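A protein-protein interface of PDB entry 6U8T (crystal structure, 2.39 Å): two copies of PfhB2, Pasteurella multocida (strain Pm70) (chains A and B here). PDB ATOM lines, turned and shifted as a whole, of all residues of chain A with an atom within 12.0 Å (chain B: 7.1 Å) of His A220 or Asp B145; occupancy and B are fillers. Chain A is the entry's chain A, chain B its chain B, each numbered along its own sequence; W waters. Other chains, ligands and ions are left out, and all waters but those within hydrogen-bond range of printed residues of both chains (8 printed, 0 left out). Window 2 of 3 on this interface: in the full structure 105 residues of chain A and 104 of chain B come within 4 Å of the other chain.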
ATOM      1  N   SER A 164     -12.346  25.737  18.168  1.00  0.00           N
ATOM      2  CA  SER A 164     -11.801  26.367  16.941  1.00  0.00           C
ATOM      3  C   SER A 164     -10.277  26.449  17.031  1.00  0.00           C
ATOM      4  O   SER A 164      -9.690  26.201  18.093  1.00  0.00           O
ATOM      5  CB  SER A 164     -12.444  27.666  16.698  1.00  0.00           C
ATOM      6  OG  SER A 164     -12.377  28.444  17.879  1.00  0.00           O
ATOM      7  N   ALA A 165      -9.641  26.686  15.904  1.00  0.00           N
ATOM      8  CA  ALA A 165      -8.170  26.729  15.786  1.00  0.00           C
ATOM      9  C   ALA A 165      -7.809  27.731  14.699  1.00  0.00           C
ATOM     10  O   ALA A 165      -8.600  27.911  13.757  1.00  0.00           O
ATOM     11  CB  ALA A 165      -7.660  25.343  15.502  1.00  0.00           C
ATOM     12  N   LEU A 166      -6.684  28.393  14.872  1.00  0.00           N
ATOM     13  CA  LEU A 166      -5.984  29.130  13.788  1.00  0.00           C
ATOM     14  C   LEU A 166      -4.590  28.524  13.665  1.00  0.00           C
ATOM     15  O   LEU A 166      -3.864  28.469  14.693  1.00  0.00           O
ATOM     16  CB  LEU A 166      -5.938  30.606  14.167  1.00  0.00           C
ATOM     17  CG  LEU A 166      -5.148  31.518  13.228  1.00  0.00           C
ATOM     18  CD1 LEU A 166      -5.839  31.716  11.890  1.00  0.00           C
ATOM     19  CD2 LEU A 166      -4.925  32.844  13.916  1.00  0.00           C
ATOM     20  N   VAL A 167      -4.252  28.007  12.497  1.00  0.00           N
ATOM     21  CA  VAL A 167      -2.859  27.557  12.249  1.00  0.00           C
ATOM     22  C   VAL A 167      -2.225  28.535  11.252  1.00  0.00           C
ATOM     23  O   VAL A 167      -2.846  28.843  10.261  1.00  0.00           O
ATOM     24  CB  VAL A 167      -2.692  26.052  11.953  1.00  0.00           C
ATOM     25  CG1 VAL A 167      -3.971  25.297  11.915  1.00  0.00           C
ATOM     26  CG2 VAL A 167      -1.755  25.717  10.793  1.00  0.00           C
ATOM     27  N   GLN A 168      -1.079  29.093  11.622  1.00  0.00           N
ATOM     28  CA  GLN A 168      -0.237  30.015  10.802  1.00  0.00           C
ATOM     29  C   GLN A 168       1.190  29.465  10.794  1.00  0.00           C
ATOM     30  O   GLN A 168       1.857  29.613  11.793  1.00  0.00           O
ATOM     31  CB  GLN A 168      -0.261  31.422  11.392  1.00  0.00           C
ATOM     32  CG  GLN A 168      -1.618  32.076  11.188  1.00  0.00           C
ATOM     33  CD  GLN A 168      -1.801  33.387  11.895  1.00  0.00           C
ATOM     34  OE1 GLN A 168      -1.390  33.554  13.044  1.00  0.00           O
ATOM     35  NE2 GLN A 168      -2.528  34.277  11.232  1.00  0.00           N
ATOM     36  N   GLY A 169       1.580  28.776   9.737  1.00  0.00           N
ATOM     37  CA  GLY A 169       2.849  28.038   9.705  1.00  0.00           C
ATOM     38  C   GLY A 169       2.852  27.018  10.807  1.00  0.00           C
ATOM     39  O   GLY A 169       1.894  26.220  10.857  1.00  0.00           O
ATOM     40  N   GLU A 170       3.864  27.064  11.682  1.00  0.00           N
ATOM     41  CA  GLU A 170       4.052  26.103  12.808  1.00  0.00           C
ATOM     42  C   GLU A 170       3.224  26.598  14.024  1.00  0.00           C
ATOM     43  O   GLU A 170       3.048  25.829  14.988  1.00  0.00           O
ATOM     44  CB  GLU A 170       5.545  25.937  13.098  1.00  0.00           C
ATOM     45  CG  GLU A 170       6.218  24.825  12.286  1.00  0.00           C
ATOM     46  CD  GLU A 170       5.559  23.430  12.391  1.00  0.00           C
ATOM     47  OE1 GLU A 170       5.552  22.770  13.496  1.00  0.00           O
ATOM     48  OE2 GLU A 170       5.086  22.938  11.327  1.00  0.00           O
ATOM     49  N   LYS A 171       2.718  27.831  14.006  1.00  0.00           N
ATOM     50  CA  LYS A 171       1.952  28.385  15.149  1.00  0.00           C
ATOM     51  C   LYS A 171       0.523  27.813  15.138  1.00  0.00           C
ATOM     52  O   LYS A 171      -0.171  27.951  14.108  1.00  0.00           O
ATOM     53  CB  LYS A 171       1.953  29.909  15.132  1.00  0.00           C
ATOM     54  CG  LYS A 171       1.353  30.515  16.392  1.00  0.00           C
ATOM     55  CD  LYS A 171       1.401  32.037  16.444  1.00  0.00           C
ATOM     56  CE  LYS A 171       0.145  32.737  16.928  1.00  0.00           C
ATOM     57  NZ  LYS A 171       0.251  33.099  18.363  1.00  0.00           N
ATOM     58  N   HIS A 187       3.491  22.443  15.552  1.00  0.00           N
ATOM     59  CA  HIS A 187       2.459  21.398  15.355  1.00  0.00           C
ATOM     60  C   HIS A 187       2.671  20.278  16.374  1.00  0.00           C
ATOM     61  O   HIS A 187       1.704  19.850  17.006  1.00  0.00           O
ATOM     62  CB  HIS A 187       2.457  20.845  13.923  1.00  0.00           C
ATOM     63  CG  HIS A 187       1.889  21.773  12.903  1.00  0.00           C
ATOM     64  ND1 HIS A 187       1.768  23.151  13.137  1.00  0.00           N
ATOM     65  CD2 HIS A 187       1.513  21.572  11.623  1.00  0.00           C
ATOM     66  CE1 HIS A 187       1.313  23.742  12.041  1.00  0.00           C
ATOM     67  NE2 HIS A 187       1.137  22.793  11.100  1.00  0.00           N
ATOM     68  N   VAL A 216     -14.592  19.173  10.672  1.00  0.00           N
ATOM     69  CA  VAL A 216     -13.715  20.377  10.649  1.00  0.00           C
ATOM     70  C   VAL A 216     -14.136  21.200   9.436  1.00  0.00           C
ATOM     71  O   VAL A 216     -14.119  20.651   8.326  1.00  0.00           O
ATOM     72  CB  VAL A 216     -12.242  19.975  10.625  1.00  0.00           C
ATOM     73  CG1 VAL A 216     -11.339  21.188  10.496  1.00  0.00           C
ATOM     74  CG2 VAL A 216     -11.890  19.179  11.875  1.00  0.00           C
ATOM     75  N   VAL A 217     -14.541  22.456   9.656  1.00  0.00           N
ATOM     76  CA  VAL A 217     -14.809  23.395   8.540  1.00  0.00           C
ATOM     77  C   VAL A 217     -13.597  24.330   8.441  1.00  0.00           C
ATOM     78  O   VAL A 217     -13.224  24.918   9.483  1.00  0.00           O
ATOM     79  CB  VAL A 217     -16.132  24.153   8.722  1.00  0.00           C
ATOM     80  CG1 VAL A 217     -16.397  25.084   7.550  1.00  0.00           C
ATOM     81  CG2 VAL A 217     -17.289  23.197   8.922  1.00  0.00           C
ATOM     82  N   ASN A 218     -13.021  24.445   7.241  1.00  0.00           N
ATOM     83  CA  ASN A 218     -11.781  25.211   6.995  1.00  0.00           C
ATOM     84  C   ASN A 218     -12.126  26.590   6.442  1.00  0.00           C
ATOM     85  O   ASN A 218     -12.879  26.656   5.488  1.00  0.00           O
ATOM     86  CB  ASN A 218     -10.850  24.418   6.065  1.00  0.00           C
ATOM     87  CG  ASN A 218     -10.170  23.276   6.780  1.00  0.00           C
ATOM     88  OD1 ASN A 218      -9.422  23.520   7.726  1.00  0.00           O
ATOM     89  ND2 ASN A 218     -10.444  22.040   6.374  1.00  0.00           N
ATOM     90  N   TYR A 219     -11.553  27.639   7.005  1.00  0.00           N
ATOM     91  CA  TYR A 219     -11.695  29.030   6.519  1.00  0.00           C
ATOM     92  C   TYR A 219     -10.314  29.605   6.194  1.00  0.00           C
ATOM     93  O   TYR A 219      -9.323  29.272   6.871  1.00  0.00           O
ATOM     94  CB  TYR A 219     -12.421  29.900   7.564  1.00  0.00           C
ATOM     95  CG  TYR A 219     -13.728  29.308   8.005  1.00  0.00           C
ATOM     96  CD1 TYR A 219     -14.904  29.507   7.302  1.00  0.00           C
ATOM     97  CD2 TYR A 219     -13.763  28.499   9.129  1.00  0.00           C
ATOM     98  CE1 TYR A 219     -16.090  28.933   7.728  1.00  0.00           C
ATOM     99  CE2 TYR A 219     -14.942  27.919   9.559  1.00  0.00           C
ATOM    100  CZ  TYR A 219     -16.114  28.153   8.870  1.00  0.00           C
ATOM    101  OH  TYR A 219     -17.281  27.585   9.302  1.00  0.00           O
ATOM    102  N   HIS A 220     -10.268  30.503   5.220  1.00  0.00           N
ATOM    103  CA  HIS A 220      -9.037  31.295   4.907  1.00  0.00           C
ATOM    104  C   HIS A 220      -8.684  32.115   6.131  1.00  0.00           C
ATOM    105  O   HIS A 220      -9.656  32.629   6.800  1.00  0.00           O
ATOM    106  CB  HIS A 220      -9.197  32.104   3.613  1.00  0.00           C
ATOM    107  CG  HIS A 220      -9.210  31.235   2.400  1.00  0.00           C
ATOM    108  ND1 HIS A 220      -8.160  30.407   2.066  1.00  0.00           N
ATOM    109  CD2 HIS A 220     -10.167  31.002   1.478  1.00  0.00           C
ATOM    110  CE1 HIS A 220      -8.477  29.711   0.971  1.00  0.00           C
ATOM    111  NE2 HIS A 220      -9.706  30.052   0.594  1.00  0.00           N
ATOM    112  N   ALA A 221      -7.397  32.208   6.458  1.00  0.00           N
ATOM    113  CA  ALA A 221      -6.904  33.043   7.588  1.00  0.00           C
ATOM    114  C   ALA A 221      -6.890  34.516   7.170  1.00  0.00           C
ATOM    115  O   ALA A 221      -6.890  35.347   8.088  1.00  0.00           O
ATOM    116  CB  ALA A 221      -5.530  32.637   8.036  1.00  0.00           C
ATOM    117  N   ILE B  46     -13.469  33.146  15.420  1.00  0.00           N
ATOM    118  CA  ILE B  46     -12.906  32.976  14.054  1.00  0.00           C
ATOM    119  C   ILE B  46     -12.962  34.336  13.332  1.00  0.00           C
ATOM    120  O   ILE B  46     -11.923  34.763  12.820  1.00  0.00           O
ATOM    121  CB  ILE B  46     -13.608  31.843  13.286  1.00  0.00           C
ATOM    122  CG1 ILE B  46     -13.252  30.496  13.891  1.00  0.00           C
ATOM    123  CG2 ILE B  46     -13.247  31.884  11.826  1.00  0.00           C
ATOM    124  CD1 ILE B  46     -14.014  29.339  13.277  1.00  0.00           C
ATOM    125  N   VAL B  50      -9.601  36.514  11.977  1.00  0.00           N
ATOM    126  CA  VAL B  50      -9.445  36.651  10.500  1.00  0.00           C
ATOM    127  C   VAL B  50      -9.535  38.137  10.160  1.00  0.00           C
ATOM    128  O   VAL B  50      -8.769  38.574   9.337  1.00  0.00           O
ATOM    129  CB  VAL B  50     -10.518  35.794   9.808  1.00  0.00           C
ATOM    130  CG1 VAL B  50     -10.819  36.237   8.392  1.00  0.00           C
ATOM    131  CG2 VAL B  50     -10.183  34.310   9.889  1.00  0.00           C
ATOM    132  N   GLY B 106     -17.149  38.640   6.772  1.00  0.00           N
ATOM    133  CA  GLY B 106     -15.989  38.731   5.876  1.00  0.00           C
ATOM    134  C   GLY B 106     -15.090  37.513   5.968  1.00  0.00           C
ATOM    135  O   GLY B 106     -14.037  37.551   5.325  1.00  0.00           O
ATOM    136  N   VAL B 107     -15.499  36.453   6.671  1.00  0.00           N
ATOM    137  CA  VAL B 107     -14.741  35.169   6.755  1.00  0.00           C
ATOM    138  C   VAL B 107     -15.041  34.354   5.496  1.00  0.00           C
ATOM    139  O   VAL B 107     -16.228  34.238   5.127  1.00  0.00           O
ATOM    140  CB  VAL B 107     -15.109  34.359   8.015  1.00  0.00           C
ATOM    141  CG1 VAL B 107     -14.315  33.072   8.077  1.00  0.00           C
ATOM    142  CG2 VAL B 107     -14.906  35.172   9.286  1.00  0.00           C
ATOM    143  N   VAL B 108     -14.014  33.807   4.857  1.00  0.00           N
ATOM    144  CA  VAL B 108     -14.134  33.124   3.523  1.00  0.00           C
ATOM    145  C   VAL B 108     -13.916  31.628   3.722  1.00  0.00           C
ATOM    146  O   VAL B 108     -12.814  31.196   4.023  1.00  0.00           O
ATOM    147  CB  VAL B 108     -13.153  33.701   2.465  1.00  0.00           C
ATOM    148  CG1 VAL B 108     -13.301  32.959   1.149  1.00  0.00           C
ATOM    149  CG2 VAL B 108     -13.346  35.193   2.262  1.00  0.00           C
ATOM    150  N   PRO B 109     -14.958  30.802   3.552  1.00  0.00           N
ATOM    151  CA  PRO B 109     -14.813  29.355   3.622  1.00  0.00           C
ATOM    152  C   PRO B 109     -13.844  28.854   2.537  1.00  0.00           C
ATOM    153  O   PRO B 109     -13.926  29.321   1.423  1.00  0.00           O
ATOM    154  CB  PRO B 109     -16.249  28.805   3.349  1.00  0.00           C
ATOM    155  CG  PRO B 109     -17.178  29.973   3.386  1.00  0.00           C
ATOM    156  CD  PRO B 109     -16.331  31.207   3.210  1.00  0.00           C
ATOM    157  N   LYS B 110     -12.987  27.902   2.864  1.00  0.00           N
ATOM    158  CA  LYS B 110     -12.096  27.250   1.867  1.00  0.00           C
ATOM    159  C   LYS B 110     -12.932  26.325   0.986  1.00  0.00           C
ATOM    160  O   LYS B 110     -13.961  25.807   1.487  1.00  0.00           O
ATOM    161  CB  LYS B 110     -10.973  26.461   2.532  1.00  0.00           C
ATOM    162  CG  LYS B 110      -9.880  27.324   3.109  1.00  0.00           C
ATOM    163  CD  LYS B 110      -8.600  26.591   3.469  1.00  0.00           C
ATOM    164  CE  LYS B 110      -7.678  27.503   4.280  1.00  0.00           C
ATOM    165  NZ  LYS B 110      -6.405  26.840   4.651  1.00  0.00           N
ATOM    166  N   GLU B 111     -12.537  26.171  -0.276  1.00  0.00           N
ATOM    167  CA  GLU B 111     -13.156  25.281  -1.280  1.00  0.00           C
ATOM    168  C   GLU B 111     -12.099  24.275  -1.732  1.00  0.00           C
ATOM    169  O   GLU B 111     -10.905  24.652  -1.800  1.00  0.00           O
ATOM    170  CB  GLU B 111     -13.679  26.057  -2.490  1.00  0.00           C
ATOM    171  CG  GLU B 111     -14.327  27.377  -2.146  1.00  0.00           C
ATOM    172  CD  GLU B 111     -15.667  27.583  -2.808  1.00  0.00           C
ATOM    173  OE1 GLU B 111     -15.689  27.790  -4.075  1.00  0.00           O
ATOM    174  OE2 GLU B 111     -16.689  27.519  -2.051  1.00  0.00           O
ATOM    175  N   ASP B 141      -3.967  20.513   9.102  1.00  0.00           N
ATOM    176  CA  ASP B 141      -3.887  20.589   7.616  1.00  0.00           C
ATOM    177  C   ASP B 141      -4.303  21.990   7.178  1.00  0.00           C
ATOM    178  O   ASP B 141      -5.348  22.466   7.614  1.00  0.00           O
ATOM    179  CB  ASP B 141      -4.780  19.554   6.926  1.00  0.00           C
ATOM    180  CG  ASP B 141      -4.574  19.437   5.412  1.00  0.00           C
ATOM    181  OD1 ASP B 141      -3.612  20.000   4.831  1.00  0.00           O
ATOM    182  OD2 ASP B 141      -5.319  18.666   4.812  1.00  0.00           O
ATOM    183  N   THR B 142      -3.497  22.647   6.353  1.00  0.00           N
ATOM    184  CA  THR B 142      -3.822  23.968   5.772  1.00  0.00           C
ATOM    185  C   THR B 142      -3.933  23.848   4.247  1.00  0.00           C
ATOM    186  O   THR B 142      -4.081  24.904   3.599  1.00  0.00           O
ATOM    187  CB  THR B 142      -2.804  25.014   6.243  1.00  0.00           C
ATOM    188  OG1 THR B 142      -1.475  24.508   6.138  1.00  0.00           O
ATOM    189  CG2 THR B 142      -3.082  25.436   7.671  1.00  0.00           C
ATOM    190  N   GLY B 143      -3.918  22.624   3.714  1.00  0.00           N
ATOM    191  CA  GLY B 143      -4.053  22.349   2.268  1.00  0.00           C
ATOM    192  C   GLY B 143      -2.957  23.000   1.445  1.00  0.00           C
ATOM    193  O   GLY B 143      -1.774  22.728   1.738  1.00  0.00           O
ATOM    194  N   SER B 144      -3.338  23.823   0.459  1.00  0.00           N
ATOM    195  CA  SER B 144      -2.449  24.622  -0.432  1.00  0.00           C
ATOM    196  C   SER B 144      -1.505  25.487   0.416  1.00  0.00           C
ATOM    197  O   SER B 144      -0.286  25.554   0.154  1.00  0.00           O
ATOM    198  CB  SER B 144      -3.274  25.600  -1.295  1.00  0.00           C
ATOM    199  OG  SER B 144      -4.182  24.994  -2.213  1.00  0.00           O
ATOM    200  N   ASP B 145      -2.136  26.189   1.377  1.00  0.00           N
ATOM    201  CA  ASP B 145      -1.574  27.362   2.099  1.00  0.00           C
ATOM    202  C   ASP B 145      -0.821  26.939   3.346  1.00  0.00           C
ATOM    203  O   ASP B 145      -0.780  25.731   3.635  1.00  0.00           O
ATOM    204  CB  ASP B 145      -2.702  28.318   2.471  1.00  0.00           C
ATOM    205  CG  ASP B 145      -3.477  28.748   1.234  1.00  0.00           C
ATOM    206  OD1 ASP B 145      -2.904  28.644   0.092  1.00  0.00           O
ATOM    207  OD2 ASP B 145      -4.640  29.164   1.405  1.00  0.00           O
ATOM    208  N   THR B 146      -0.261  27.923   4.060  1.00  0.00           N
ATOM    209  CA  THR B 146       0.461  27.706   5.348  1.00  0.00           C
ATOM    210  C   THR B 146      -0.439  28.113   6.518  1.00  0.00           C
ATOM    211  O   THR B 146      -0.082  27.787   7.664  1.00  0.00           O
ATOM    212  CB  THR B 146       1.816  28.416   5.371  1.00  0.00           C
ATOM    213  OG1 THR B 146       1.539  29.807   5.457  1.00  0.00           O
ATOM    214  CG2 THR B 146       2.670  28.136   4.152  1.00  0.00           C
ATOM    215  N   ALA B 147      -1.583  28.736   6.251  1.00  0.00           N
ATOM    216  CA  ALA B 147      -2.503  29.285   7.263  1.00  0.00           C
ATOM    217  C   ALA B 147      -3.946  28.813   7.015  1.00  0.00           C
ATOM    218  O   ALA B 147      -4.346  28.605   5.847  1.00  0.00           O
ATOM    219  CB  ALA B 147      -2.400  30.792   7.254  1.00  0.00           C
ATOM    220  N   GLY B 148      -4.707  28.692   8.097  1.00  0.00           N
ATOM    221  CA  GLY B 148      -6.173  28.473   8.059  1.00  0.00           C
ATOM    222  C   GLY B 148      -6.802  28.461   9.437  1.00  0.00           C
ATOM    223  O   GLY B 148      -6.145  28.094  10.423  1.00  0.00           O
ATOM    224  N   ALA B 149      -8.042  28.911   9.488  1.00  0.00           N
ATOM    225  CA  ALA B 149      -8.920  28.896  10.666  1.00  0.00           C
ATOM    226  C   ALA B 149      -9.887  27.711  10.536  1.00  0.00           C
ATOM    227  O   ALA B 149     -10.277  27.388   9.406  1.00  0.00           O
ATOM    228  CB  ALA B 149      -9.654  30.221  10.723  1.00  0.00           C
HETATM  229  O   HOH W   1      -0.456  22.912   8.114  1.00  0.00           O
HETATM  230  O   HOH W   2       1.013  25.178   8.431  1.00  0.00           O
HETATM  231  O   HOH W   3     -11.451  34.172   6.013  1.00  0.00           O
HETATM  232  O   HOH W   4      -5.647  30.915   4.259  1.00  0.00           O
HETATM  233  O   HOH W   5     -10.648  27.885  -1.385  1.00  0.00           O
HETATM  234  O   HOH W   6      -7.236  24.610   5.949  1.00  0.00           O
HETATM  235  O   HOH W   7     -14.983  25.716   4.032  1.00  0.00           O
HETATM  236  O   HOH W   8     -12.338  29.823  -1.367  1.00  0.00           O
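Gly B148 touches Leu A166 (O to CA, 3.5 Å).
Thr B142 touches Val A167 (CG2 to CG2, 3.4 Å).
Gln A168 touches Thr B146 (C to O, 3.8 Å).
O of Asn A218 touches C of Pro B109, at 3.8 Å.
O of Ala B149 touches CA of Asn A218, at 3.6 Å.
Tyr A219 touches Pro B109 (CD1 to CA, 3.7 Å).
Tyr A219 touches Lys B110 (O to CE, 3.5 Å).
CG2 of Val B50 touches O of His A220 (3.6 Å).
His A220 touches Lys B110.
His A220 touches Asp B145 (ND1 to OD2, 3.8 Å).
No position is printed for both chains.
Of the 24 pairs that touch across the chains among the printed residues, none has its exchanged pair printed and touching as well.
Of the 17 printed residues of chain B, 11 touch a printed residue of chain A.
Printed residues of chain B that touch a printed residue of chain A: Val B50, Val B107, Val B108, Pro B109, Lys B110, Thr B142, Asp B145, Thr B146, Ala B147, Gly B148 and Ala B149.
Hydrophobic or aromatic side chains of chain B that line the printed part of chain A: Val B50, Val B107, Val B108, Ala B147 and Ala B149.
Of the 15 printed residues of chain A, 10 touch a printed residue of chain B.
Printed residues of chain A that touch a printed residue of chain B: Ala A165, Leu A166, Val A167, Gln A168, Gly A169, Val A217, Asn A218, Tyr A219, His A220 and Ala A221.
Among the printed residues, no Asp or Glu carboxylate lies within 4 Å of a Lys or Arg side-chain nitrogen of the other chain.
Of the printed residues of chain B, Ala A165 touches Ala B149.
Of the printed residues of chain B, Val A167 touches Thr B142 (3.4 Å), Thr B146 (3.9 Å), Ala B147 (3.0 Å) and Gly B148 (2.8 Å).
Of the printed residues of chain B, Gly A169 touches Thr B146.
Lys A171 touches none of the printed residues of chain B.
Of the printed residues of chain B, Val A217 touches Ala B149.
Of chain B, only Val B50, Val B108, Lys B110 and Asp B145 come within 4 Å of His A220.
Val B50 touches just these residues of chain A: His A220 and Ala A221.
Pro B109 touches two residues of chain A.
No residue of chain A comes within 4 Å of Glu B111.
No residue of chain A comes within 4 Å of Gly B143.
No residue of chain A comes within 4 Å of Ser B144.
Of chain A, only His A220 (3.8 Å) comes within 4 Å of Asp B145.
Thr B146 touches just these residues of chain A: Val A167, Gln A168 and Gly A169.
Of chain A, only Val A167 (3.0 Å) and Ala A221 (3.7 Å) come within 4 Å of Ala B147.
Of the printed residues of chain A, Ala B149 touches Ala A165 (3.3 Å), Val A217 (3.8 Å), Asn A218 (3.6 Å) and Tyr A219 (2.7 Å).
The nearest residue of chain B that does not touch His A220 is Pro B109 (4.1 Å).
The nearest residue of chain A that does not touch Asp B145 is Ala A221 (6.5 Å).
The nearest printed residue of chain B that does not touch Gln A168 is Ala B147 (4.2 Å).
Water W3 bridges O of His A220 and N of Val B108.
Water W6 lies within hydrogen-bond range of the side-chain amino group of Lys B110 (2.7 Å), the side-chain amide oxygen of Asn A218 (3.0 Å) and the backbone carbonyl oxygen of Asp B141 (3.3 Å).
Water W1 bridges OG1 of Thr B142 (2.7 Å) and NE2 of His A187 (3.4 Å).
Water W5 lies within hydrogen-bond range of the backbone NH (N) of Glu B111 (2.8 Å) and a ring nitrogen (NE2) of His A220 (3.1 Å).
Water W4 lies within hydrogen-bond range of O of Ala B147, N of Ala A221, ND1 of His A220 and OD2 of Asp B145.
Water W8 lies within hydrogen-bond range of the backbone carbonyl oxygen (O) of Pro B109 (3.2 Å) and a ring nitrogen (NE2) of His A220 (3.3 Å).
The backbone NH (N) of His A220 is in hydrogen-bond range of the backbone carbonyl oxygen (O) of Val B108.
The backbone carbonyl oxygen (O) of Asn A218 sits at hydrogen-bond distance from the backbone NH (N) of Lys B110 (2.9 Å).
The backbone NH (N) of Gly A169 sits at hydrogen-bond distance from the backbone carbonyl oxygen (O) of Thr B146 (2.8 Å).
N of Tyr A219 lies within hydrogen-bond range of O of Ala B149 (2.7 Å).
The backbone NH of Val A167 sits at hydrogen-bond distance from the backbone carbonyl oxygen of Gly B148.
The side-chain amino group of Lys B110 sits at hydrogen-bond distance from the backbone carbonyl oxygen of Thr B142 (3.2 Å).
The side-chain amino group (NZ) of Lys B110 sits at hydrogen-bond distance from the backbone carbonyl oxygen (O) of Ala B147 (3.0 Å).
The side-chain hydroxyl of Thr B142 lies within hydrogen-bond range of the backbone carbonyl oxygen of Asp B145 (2.9 Å).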
